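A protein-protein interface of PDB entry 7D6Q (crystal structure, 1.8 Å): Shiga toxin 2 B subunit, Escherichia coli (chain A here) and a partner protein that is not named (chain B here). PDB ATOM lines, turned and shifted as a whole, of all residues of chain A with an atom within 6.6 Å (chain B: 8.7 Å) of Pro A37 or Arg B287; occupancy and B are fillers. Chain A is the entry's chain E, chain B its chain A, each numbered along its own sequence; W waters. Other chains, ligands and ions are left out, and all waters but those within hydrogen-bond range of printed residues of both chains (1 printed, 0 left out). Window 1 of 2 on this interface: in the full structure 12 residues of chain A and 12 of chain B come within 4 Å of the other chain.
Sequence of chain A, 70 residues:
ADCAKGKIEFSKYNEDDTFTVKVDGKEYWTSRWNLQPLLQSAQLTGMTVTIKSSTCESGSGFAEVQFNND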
ATOM      1  N   PHE A  19     -14.151 -15.426  12.472  1.00  0.00           N
ATOM      2  CA  PHE A  19     -14.788 -16.707  12.163  1.00  0.00           C
ATOM      3  C   PHE A  19     -15.468 -17.188  13.438  1.00  0.00           C
ATOM      4  O   PHE A  19     -14.792 -17.534  14.411  1.00  0.00           O
ATOM      5  CB  PHE A  19     -13.759 -17.723  11.656  1.00  0.00           C
ATOM      6  CG  PHE A  19     -14.354 -18.977  11.070  1.00  0.00           C
ATOM      7  CD1 PHE A  19     -14.840 -18.987   9.768  1.00  0.00           C
ATOM      8  CD2 PHE A  19     -14.398 -20.154  11.812  1.00  0.00           C
ATOM      9  CE1 PHE A  19     -15.378 -20.150   9.222  1.00  0.00           C
ATOM     10  CE2 PHE A  19     -14.934 -21.326  11.270  1.00  0.00           C
ATOM     11  CZ  PHE A  19     -15.422 -21.323   9.974  1.00  0.00           C
ATOM     12  N   ARG A  32      -7.692 -16.584  13.474  1.00  0.00           N
ATOM     13  CA  ARG A  32      -6.658 -17.471  12.952  1.00  0.00           C
ATOM     14  C   ARG A  32      -7.211 -18.207  11.736  1.00  0.00           C
ATOM     15  O   ARG A  32      -8.090 -19.064  11.875  1.00  0.00           O
ATOM     16  CB  ARG A  32      -6.216 -18.467  14.024  1.00  0.00           C
ATOM     17  CG  ARG A  32      -5.886 -17.846  15.386  1.00  0.00           C
ATOM     18  CD  ARG A  32      -4.602 -17.009  15.361  1.00  0.00           C
ATOM     19  NE  ARG A  32      -4.463 -16.275  16.617  1.00  0.00           N
ATOM     20  CZ  ARG A  32      -3.637 -16.616  17.601  1.00  0.00           C
ATOM     21  NH1 ARG A  32      -2.840 -17.668  17.472  1.00  0.00           N
ATOM     22  NH2 ARG A  32      -3.600 -15.897  18.715  1.00  0.00           N
ATOM     23  N   TRP A  33      -6.717 -17.878  10.541  1.00  0.00           N
ATOM     24  CA  TRP A  33      -7.197 -18.596   9.364  1.00  0.00           C
ATOM     25  C   TRP A  33      -6.847 -20.075   9.434  1.00  0.00           C
ATOM     26  O   TRP A  33      -7.573 -20.906   8.870  1.00  0.00           O
ATOM     27  CB  TRP A  33      -6.630 -17.983   8.079  1.00  0.00           C
ATOM     28  CG  TRP A  33      -7.379 -16.762   7.575  1.00  0.00           C
ATOM     29  CD1 TRP A  33      -8.105 -15.872   8.317  1.00  0.00           C
ATOM     30  CD2 TRP A  33      -7.450 -16.304   6.214  1.00  0.00           C
ATOM     31  NE1 TRP A  33      -8.630 -14.886   7.494  1.00  0.00           N
ATOM     32  CE2 TRP A  33      -8.241 -15.130   6.203  1.00  0.00           C
ATOM     33  CE3 TRP A  33      -6.930 -16.775   5.009  1.00  0.00           C
ATOM     34  CZ2 TRP A  33      -8.522 -14.423   5.024  1.00  0.00           C
ATOM     35  CZ3 TRP A  33      -7.203 -16.067   3.840  1.00  0.00           C
ATOM     36  CH2 TRP A  33      -7.996 -14.907   3.857  1.00  0.00           C
ATOM     37  N   ASN A  34      -5.745 -20.426  10.118  1.00  0.00           N
ATOM     38  CA  ASN A  34      -5.420 -21.839  10.309  1.00  0.00           C
ATOM     39  C   ASN A  34      -6.624 -22.605  10.821  1.00  0.00           C
ATOM     40  O   ASN A  34      -6.816 -23.778  10.486  1.00  0.00           O
ATOM     41  CB  ASN A  34      -4.281 -22.014  11.322  1.00  0.00           C
ATOM     42  CG  ASN A  34      -2.902 -21.836  10.717  1.00  0.00           C
ATOM     43  OD1 ASN A  34      -2.728 -21.883   9.496  1.00  0.00           O
ATOM     44  ND2 ASN A  34      -1.906 -21.614  11.584  1.00  0.00           N
ATOM     45  N   LEU A  35      -7.426 -21.967  11.672  1.00  0.00           N
ATOM     46  CA  LEU A  35      -8.522 -22.674  12.319  1.00  0.00           C
ATOM     47  C   LEU A  35      -9.759 -22.799  11.439  1.00  0.00           C
ATOM     48  O   LEU A  35     -10.632 -23.620  11.746  1.00  0.00           O
ATOM     49  CB  LEU A  35      -8.875 -21.974  13.636  1.00  0.00           C
ATOM     50  CG  LEU A  35      -7.975 -22.404  14.796  1.00  0.00           C
ATOM     51  CD1 LEU A  35      -8.188 -21.499  16.001  1.00  0.00           C
ATOM     52  CD2 LEU A  35      -8.238 -23.869  15.150  1.00  0.00           C
ATOM     53  N   GLN A  36      -9.866 -22.038  10.342  1.00  0.00           N
ATOM     54  CA  GLN A  36     -11.094 -22.143   9.552  1.00  0.00           C
ATOM     55  C   GLN A  36     -11.282 -23.526   8.939  1.00  0.00           C
ATOM     56  O   GLN A  36     -12.347 -24.131   9.167  1.00  0.00           O
ATOM     57  CB  GLN A  36     -11.150 -21.025   8.507  1.00  0.00           C
ATOM     58  CG  GLN A  36     -11.292 -19.654   9.155  1.00  0.00           C
ATOM     59  CD  GLN A  36     -11.611 -18.561   8.158  1.00  0.00           C
ATOM     60  OE1 GLN A  36     -12.150 -18.820   7.077  1.00  0.00           O
ATOM     61  NE2 GLN A  36     -11.292 -17.320   8.525  1.00  0.00           N
ATOM     62  N   PRO A  37     -10.334 -24.091   8.176  1.00  0.00           N
ATOM     63  CA  PRO A  37     -10.566 -25.458   7.665  1.00  0.00           C
ATOM     64  C   PRO A  37     -10.637 -26.492   8.772  1.00  0.00           C
ATOM     65  O   PRO A  37     -11.401 -27.456   8.665  1.00  0.00           O
ATOM     66  CB  PRO A  37      -9.364 -25.703   6.742  1.00  0.00           C
ATOM     67  CG  PRO A  37      -8.296 -24.732   7.236  1.00  0.00           C
ATOM     68  CD  PRO A  37      -9.067 -23.525   7.669  1.00  0.00           C
ATOM     69  N   LEU A  38      -9.847 -26.319   9.835  1.00  0.00           N
ATOM     70  CA  LEU A  38      -9.896 -27.267  10.947  1.00  0.00           C
ATOM     71  C   LEU A  38     -11.273 -27.273  11.593  1.00  0.00           C
ATOM     72  O   LEU A  38     -11.859 -28.337  11.822  1.00  0.00           O
ATOM     73  CB  LEU A  38      -8.819 -26.929  11.983  1.00  0.00           C
ATOM     74  CG  LEU A  38      -7.388 -26.923  11.445  1.00  0.00           C
ATOM     75  CD1 LEU A  38      -6.416 -26.435  12.521  1.00  0.00           C
ATOM     76  CD2 LEU A  38      -6.971 -28.293  10.910  1.00  0.00           C
ATOM     77  N   LEU A  39     -11.821 -26.085  11.868  1.00  0.00           N
ATOM     78  CA  LEU A  39     -13.139 -26.019  12.494  1.00  0.00           C
ATOM     79  C   LEU A  39     -14.234 -26.504  11.546  1.00  0.00           C
ATOM     80  O   LEU A  39     -15.121 -27.267  11.952  1.00  0.00           O
ATOM     81  CB  LEU A  39     -13.421 -24.594  12.975  1.00  0.00           C
ATOM     82  CG  LEU A  39     -12.618 -24.113  14.196  1.00  0.00           C
ATOM     83  CD1 LEU A  39     -12.737 -22.604  14.366  1.00  0.00           C
ATOM     84  CD2 LEU A  39     -13.056 -24.839  15.490  1.00  0.00           C
ATOM     85  N   GLN A  40     -14.199 -26.080  10.278  1.00  0.00           N
ATOM     86  CA  GLN A  40     -15.251 -26.517   9.362  1.00  0.00           C
ATOM     87  C   GLN A  40     -15.225 -28.027   9.159  1.00  0.00           C
ATOM     88  O   GLN A  40     -16.280 -28.674   9.163  1.00  0.00           O
ATOM     89  CB  GLN A  40     -15.152 -25.805   8.016  1.00  0.00           C
ATOM     90  CG  GLN A  40     -16.448 -26.057   7.217  1.00  0.00           C
ATOM     91  CD  GLN A  40     -16.281 -25.896   5.728  1.00  0.00           C
ATOM     92  OE1 GLN A  40     -15.308 -26.382   5.135  1.00  0.00           O
ATOM     93  NE2 GLN A  40     -17.246 -25.223   5.102  1.00  0.00           N
ATOM     94  N   SER A  41     -14.034 -28.611   8.988  1.00  0.00           N
ATOM     95  CA  SER A  41     -13.943 -30.063   8.924  1.00  0.00           C
ATOM     96  C   SER A  41     -14.547 -30.685  10.175  1.00  0.00           C
ATOM     97  O   SER A  41     -15.358 -31.621  10.087  1.00  0.00           O
ATOM     98  CB  SER A  41     -12.489 -30.498   8.744  1.00  0.00           C
ATOM     99  OG  SER A  41     -12.033 -30.130   7.451  1.00  0.00           O
ATOM    100  N   ALA A  42     -14.209 -30.128  11.341  1.00  0.00           N
ATOM    101  CA  ALA A  42     -14.777 -30.652  12.579  1.00  0.00           C
ATOM    102  C   ALA A  42     -16.295 -30.560  12.546  1.00  0.00           C
ATOM    103  O   ALA A  42     -16.990 -31.484  12.982  1.00  0.00           O
ATOM    104  CB  ALA A  42     -14.215 -29.891  13.784  1.00  0.00           C
ATOM    105  N   LEU A  44     -18.289 -30.571   9.817  1.00  0.00           N
ATOM    106  CA  LEU A  44     -18.994 -31.406   8.860  1.00  0.00           C
ATOM    107  C   LEU A  44     -18.831 -32.889   9.155  1.00  0.00           C
ATOM    108  O   LEU A  44     -19.608 -33.696   8.640  1.00  0.00           O
ATOM    109  CB  LEU A  44     -18.541 -31.078   7.438  1.00  0.00           C
ATOM    110  CG  LEU A  44     -17.111 -31.393   7.012  1.00  0.00           C
ATOM    111  CD1 LEU A  44     -17.051 -32.764   6.357  1.00  0.00           C
ATOM    112  CD2 LEU A  44     -16.665 -30.314   6.029  1.00  0.00           C
ATOM    113  N   THR B 280     -18.177 -36.643   2.167  1.00  0.00           N
ATOM    114  CA  THR B 280     -17.621 -36.201   3.445  1.00  0.00           C
ATOM    115  C   THR B 280     -16.092 -36.182   3.393  1.00  0.00           C
ATOM    116  O   THR B 280     -15.439 -35.183   3.766  1.00  0.00           O
ATOM    117  CB  THR B 280     -18.112 -37.123   4.569  1.00  0.00           C
ATOM    118  OG1 THR B 280     -19.548 -37.076   4.647  1.00  0.00           O
ATOM    119  CG2 THR B 280     -17.518 -36.712   5.902  1.00  0.00           C
ATOM    120  N   ALA B 281     -15.502 -37.291   2.926  1.00  0.00           N
ATOM    121  CA  ALA B 281     -14.050 -37.346   2.790  1.00  0.00           C
ATOM    122  C   ALA B 281     -13.558 -36.243   1.863  1.00  0.00           C
ATOM    123  O   ALA B 281     -12.616 -35.515   2.196  1.00  0.00           O
ATOM    124  CB  ALA B 281     -13.614 -38.727   2.286  1.00  0.00           C
ATOM    125  N   ALA B 282     -14.217 -36.074   0.709  1.00  0.00           N
ATOM    126  CA  ALA B 282     -13.817 -35.018  -0.220  1.00  0.00           C
ATOM    127  C   ALA B 282     -13.853 -33.649   0.446  1.00  0.00           C
ATOM    128  O   ALA B 282     -13.012 -32.789   0.156  1.00  0.00           O
ATOM    129  CB  ALA B 282     -14.726 -35.025  -1.452  1.00  0.00           C
ATOM    130  N   ALA B 283     -14.822 -33.428   1.340  1.00  0.00           N
ATOM    131  CA  ALA B 283     -14.982 -32.120   1.966  1.00  0.00           C
ATOM    132  C   ALA B 283     -13.928 -31.817   3.020  1.00  0.00           C
ATOM    133  O   ALA B 283     -13.825 -30.654   3.434  1.00  0.00           O
ATOM    134  CB  ALA B 283     -16.369 -31.996   2.596  1.00  0.00           C
ATOM    135  N   PHE B 284     -13.168 -32.807   3.508  1.00  0.00           N
ATOM    136  CA  PHE B 284     -11.983 -32.418   4.283  1.00  0.00           C
ATOM    137  C   PHE B 284     -10.654 -32.746   3.601  1.00  0.00           C
ATOM    138  O   PHE B 284      -9.597 -32.480   4.179  1.00  0.00           O
ATOM    139  CB  PHE B 284     -12.027 -32.986   5.718  1.00  0.00           C
ATOM    140  CG  PHE B 284     -11.983 -34.495   5.818  1.00  0.00           C
ATOM    141  CD1 PHE B 284     -10.782 -35.186   5.759  1.00  0.00           C
ATOM    142  CD2 PHE B 284     -13.145 -35.213   6.048  1.00  0.00           C
ATOM    143  CE1 PHE B 284     -10.744 -36.587   5.890  1.00  0.00           C
ATOM    144  CE2 PHE B 284     -13.124 -36.601   6.176  1.00  0.00           C
ATOM    145  CZ  PHE B 284     -11.928 -37.292   6.103  1.00  0.00           C
ATOM    146  N   LEU B 285     -10.672 -33.240   2.362  1.00  0.00           N
ATOM    147  CA  LEU B 285      -9.456 -33.485   1.597  1.00  0.00           C
ATOM    148  C   LEU B 285      -9.281 -32.478   0.465  1.00  0.00           C
ATOM    149  O   LEU B 285      -8.515 -32.724  -0.473  1.00  0.00           O
ATOM    150  CB  LEU B 285      -9.457 -34.911   1.044  1.00  0.00           C
ATOM    151  CG  LEU B 285      -9.541 -36.006   2.115  1.00  0.00           C
ATOM    152  CD1 LEU B 285      -9.789 -37.369   1.476  1.00  0.00           C
ATOM    153  CD2 LEU B 285      -8.264 -36.026   2.971  1.00  0.00           C
ATOM    154  N   ASN B 286      -9.987 -31.351   0.525  1.00  0.00           N
ATOM    155  CA  ASN B 286      -9.925 -30.337  -0.520  1.00  0.00           C
ATOM    156  C   ASN B 286      -9.178 -29.092  -0.053  1.00  0.00           C
ATOM    157  O   ASN B 286      -9.355 -28.014  -0.631  1.00  0.00           O
ATOM    158  CB  ASN B 286     -11.336 -29.976  -0.995  1.00  0.00           C
ATOM    159  CG  ASN B 286     -12.138 -29.262   0.070  1.00  0.00           C
ATOM    160  OD1 ASN B 286     -11.774 -29.289   1.248  1.00  0.00           O
ATOM    161  ND2 ASN B 286     -13.233 -28.607  -0.333  1.00  0.00           N
ATOM    162  N   ARG B 287      -8.341 -29.224   0.972  1.00  0.00           N
ATOM    163  CA  ARG B 287      -7.576 -28.101   1.506  1.00  0.00           C
ATOM    164  C   ARG B 287      -6.198 -28.064   0.858  1.00  0.00           C
ATOM    165  O   ARG B 287      -5.576 -29.110   0.651  1.00  0.00           O
ATOM    166  CB  ARG B 287      -7.432 -28.227   3.026  1.00  0.00           C
ATOM    167  CG  ARG B 287      -8.667 -27.806   3.850  1.00  0.00           C
ATOM    168  CD  ARG B 287      -9.765 -28.888   3.894  1.00  0.00           C
ATOM    169  NE  ARG B 287     -10.773 -28.580   4.917  1.00  0.00           N
ATOM    170  CZ  ARG B 287     -11.962 -28.024   4.673  1.00  0.00           C
ATOM    171  NH1 ARG B 287     -12.328 -27.699   3.433  1.00  0.00           N
ATOM    172  NH2 ARG B 287     -12.795 -27.776   5.685  1.00  0.00           N
ATOM    173  N   LYS B 288      -5.712 -26.862   0.548  1.00  0.00           N
ATOM    174  CA  LYS B 288      -4.347 -26.746   0.049  1.00  0.00           C
ATOM    175  C   LYS B 288      -3.371 -26.655   1.224  1.00  0.00           C
ATOM    176  O   LYS B 288      -3.741 -26.789   2.396  1.00  0.00           O
ATOM    177  CB  LYS B 288      -4.188 -25.548  -0.889  1.00  0.00           C
ATOM    178  CG  LYS B 288      -4.153 -24.198  -0.210  1.00  0.00           C
ATOM    179  CD  LYS B 288      -3.918 -23.086  -1.259  1.00  0.00           C
ATOM    180  CE  LYS B 288      -4.042 -21.697  -0.654  1.00  0.00           C
ATOM    181  NZ  LYS B 288      -3.678 -20.625  -1.626  1.00  0.00           N
ATOM    182  N   SER B 289      -2.095 -26.444   0.912  1.00  0.00           N
ATOM    183  CA  SER B 289      -1.079 -26.419   1.956  1.00  0.00           C
ATOM    184  C   SER B 289      -1.418 -25.323   2.960  1.00  0.00           C
ATOM    185  O   SER B 289      -1.721 -24.190   2.578  1.00  0.00           O
ATOM    186  CB  SER B 289       0.305 -26.187   1.338  1.00  0.00           C
ATOM    187  OG  SER B 289       1.241 -25.713   2.302  1.00  0.00           O
ATOM    188  N   GLN B 290      -1.367 -25.669   4.248  1.00  0.00           N
ATOM    189  CA  GLN B 290      -1.876 -24.781   5.290  1.00  0.00           C
ATOM    190  C   GLN B 290      -1.129 -23.446   5.329  1.00  0.00           C
ATOM    191  O   GLN B 290      -1.748 -22.379   5.473  1.00  0.00           O
ATOM    192  CB  GLN B 290      -1.789 -25.491   6.649  1.00  0.00           C
ATOM    193  CG  GLN B 290      -2.367 -24.706   7.826  1.00  0.00           C
ATOM    194  CD  GLN B 290      -3.866 -24.887   7.977  1.00  0.00           C
ATOM    195  OE1 GLN B 290      -4.607 -24.902   6.990  1.00  0.00           O
ATOM    196  NE2 GLN B 290      -4.327 -25.001   9.222  1.00  0.00           N
ATOM    197  N   TYR B 293      -2.321 -21.339   2.574  1.00  0.00           N
ATOM    198  CA  TYR B 293      -3.693 -20.902   2.811  1.00  0.00           C
ATOM    199  C   TYR B 293      -3.734 -19.706   3.749  1.00  0.00           C
ATOM    200  O   TYR B 293      -4.361 -18.675   3.454  1.00  0.00           O
ATOM    201  CB  TYR B 293      -4.493 -22.060   3.408  1.00  0.00           C
ATOM    202  CG  TYR B 293      -5.918 -21.720   3.807  1.00  0.00           C
ATOM    203  CD1 TYR B 293      -6.931 -21.638   2.849  1.00  0.00           C
ATOM    204  CD2 TYR B 293      -6.259 -21.525   5.144  1.00  0.00           C
ATOM    205  CE1 TYR B 293      -8.252 -21.350   3.219  1.00  0.00           C
ATOM    206  CE2 TYR B 293      -7.579 -21.249   5.521  1.00  0.00           C
ATOM    207  CZ  TYR B 293      -8.564 -21.160   4.559  1.00  0.00           C
ATOM    208  OH  TYR B 293      -9.874 -20.891   4.940  1.00  0.00           O
ATOM    209  N   THR B 294      -3.076 -19.832   4.896  1.00  0.00           N
ATOM    210  CA  THR B 294      -3.201 -18.815   5.927  1.00  0.00           C
ATOM    211  C   THR B 294      -2.446 -17.545   5.562  1.00  0.00           C
ATOM    212  O   THR B 294      -2.897 -16.444   5.911  1.00  0.00           O
ATOM    213  CB  THR B 294      -2.727 -19.400   7.258  1.00  0.00           C
ATOM    214  OG1 THR B 294      -3.646 -20.423   7.636  1.00  0.00           O
ATOM    215  CG2 THR B 294      -2.662 -18.345   8.350  1.00  0.00           C
HETATM  216  O   HOH W   1      -9.278 -29.898   7.411  1.00  0.00           O
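Among the printed residues, merely in contact across the chains: Trp A33 with Tyr B293 (3.4 Å), Trp A33 with Thr B294 (3.7 Å), Gln A36 with Tyr B293 (3.7 Å), Pro A37 with Gln B290 (3.7 Å), Pro A37 with Tyr B293 (3.5 Å), Ser A41 with Phe B284 (3.3 Å), Leu A44 with Thr B280 (3.9 Å) and Leu A44 with Ala B283 (3.8 Å).
The backbone carbonyl oxygen (O) of Ala B283 lies close to the side-chain amide oxygen (OD1) of Asn B286, at 3.3 Å.
The guanidinium group (NH1) of Arg B287 sits at hydrogen-bond distance from the backbone carbonyl oxygen (O) of Ala B283 (3.3 Å).
OD1 of Asn B286 is in hydrogen-bond range of NH1 of Arg B287, 2.8 Å away.
The backbone carbonyl oxygen (O) of Gln B290 is in hydrogen-bond range of the side-chain hydroxyl (OG1) of Thr B294.
The side-chain hydroxyl of Ser A41 sits at hydrogen-bond distance from the backbone carbonyl oxygen of Pro A37 (3.0 Å).
Water W1 lies within hydrogen-bond range of the side-chain hydroxyl of Ser A41 (2.8 Å), the guanidinium group of Arg B287 (3.2 Å) and the backbone carbonyl oxygen of Pro A37 (3.5 Å).
O of Pro A37 sits at hydrogen-bond distance from NH2 of Arg B287 (3.3 Å).
The side-chain amide oxygen of Gln A40 sits at hydrogen-bond distance from the guanidinium group of Arg B287, at 2.9 Å.
OG of Ser A41 sits at hydrogen-bond distance from NH2 of Arg B287 (3.0 Å).
The side-chain amide nitrogen (NE2) of Gln B290 sits at hydrogen-bond distance from the backbone carbonyl oxygen (O) of Asn A34.
OD1 of Asn A34 is in hydrogen-bond range of OG1 of Thr B294 (2.5 Å).
Of the 13 printed residues of chain B, 7 touch a printed residue of chain A.
Printed residues of chain B that touch a printed residue of chain A: Thr B280, Ala B283, Phe B284, Arg B287, Gln B290, Tyr B293 and Thr B294.
Of the 13 printed residues of chain A, 7 touch a printed residue of chain B.
Hydrophobic or aromatic side chains of chain A that line the printed part of chain B: Trp A33, Pro A37 and Leu A44.
Among the printed residues, 13 pairs touch across the chains.
Among the printed residues, no Asp or Glu carboxylate lies within 4 Å of a Lys or Arg side-chain nitrogen of the other chain.
Pro A37 touches just these residues of chain B: Arg B287, Gln B290 and Tyr B293.
Arg B287 touches just these residues of chain A: Pro A37, Gln A40 and Ser A41.
Printed residues of chain A within 4 Å of Tyr B293: Trp A33 (3.4 Å), Gln A36 (3.7 Å) and Pro A37 (3.5 Å).
Of the printed residues of chain B, Gln A40 touches Arg B287.
Printed residues of chain A within 4 Å of Phe B284: Ser A41 (3.3 Å).
Of the printed residues of chain B, Asn A34 touches Gln B290 and Thr B294.
Lys B288 touches none of the printed residues of chain A.
The nearest residue of chain B that does not touch Pro A37 is Thr B294 (6.2 Å).
The nearest residue of chain A that does not touch Arg B287 is Leu A44 (4.6 Å).
The nearest printed residue of chain B that does not touch Trp A33 is Gln B290 (5.2 Å).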
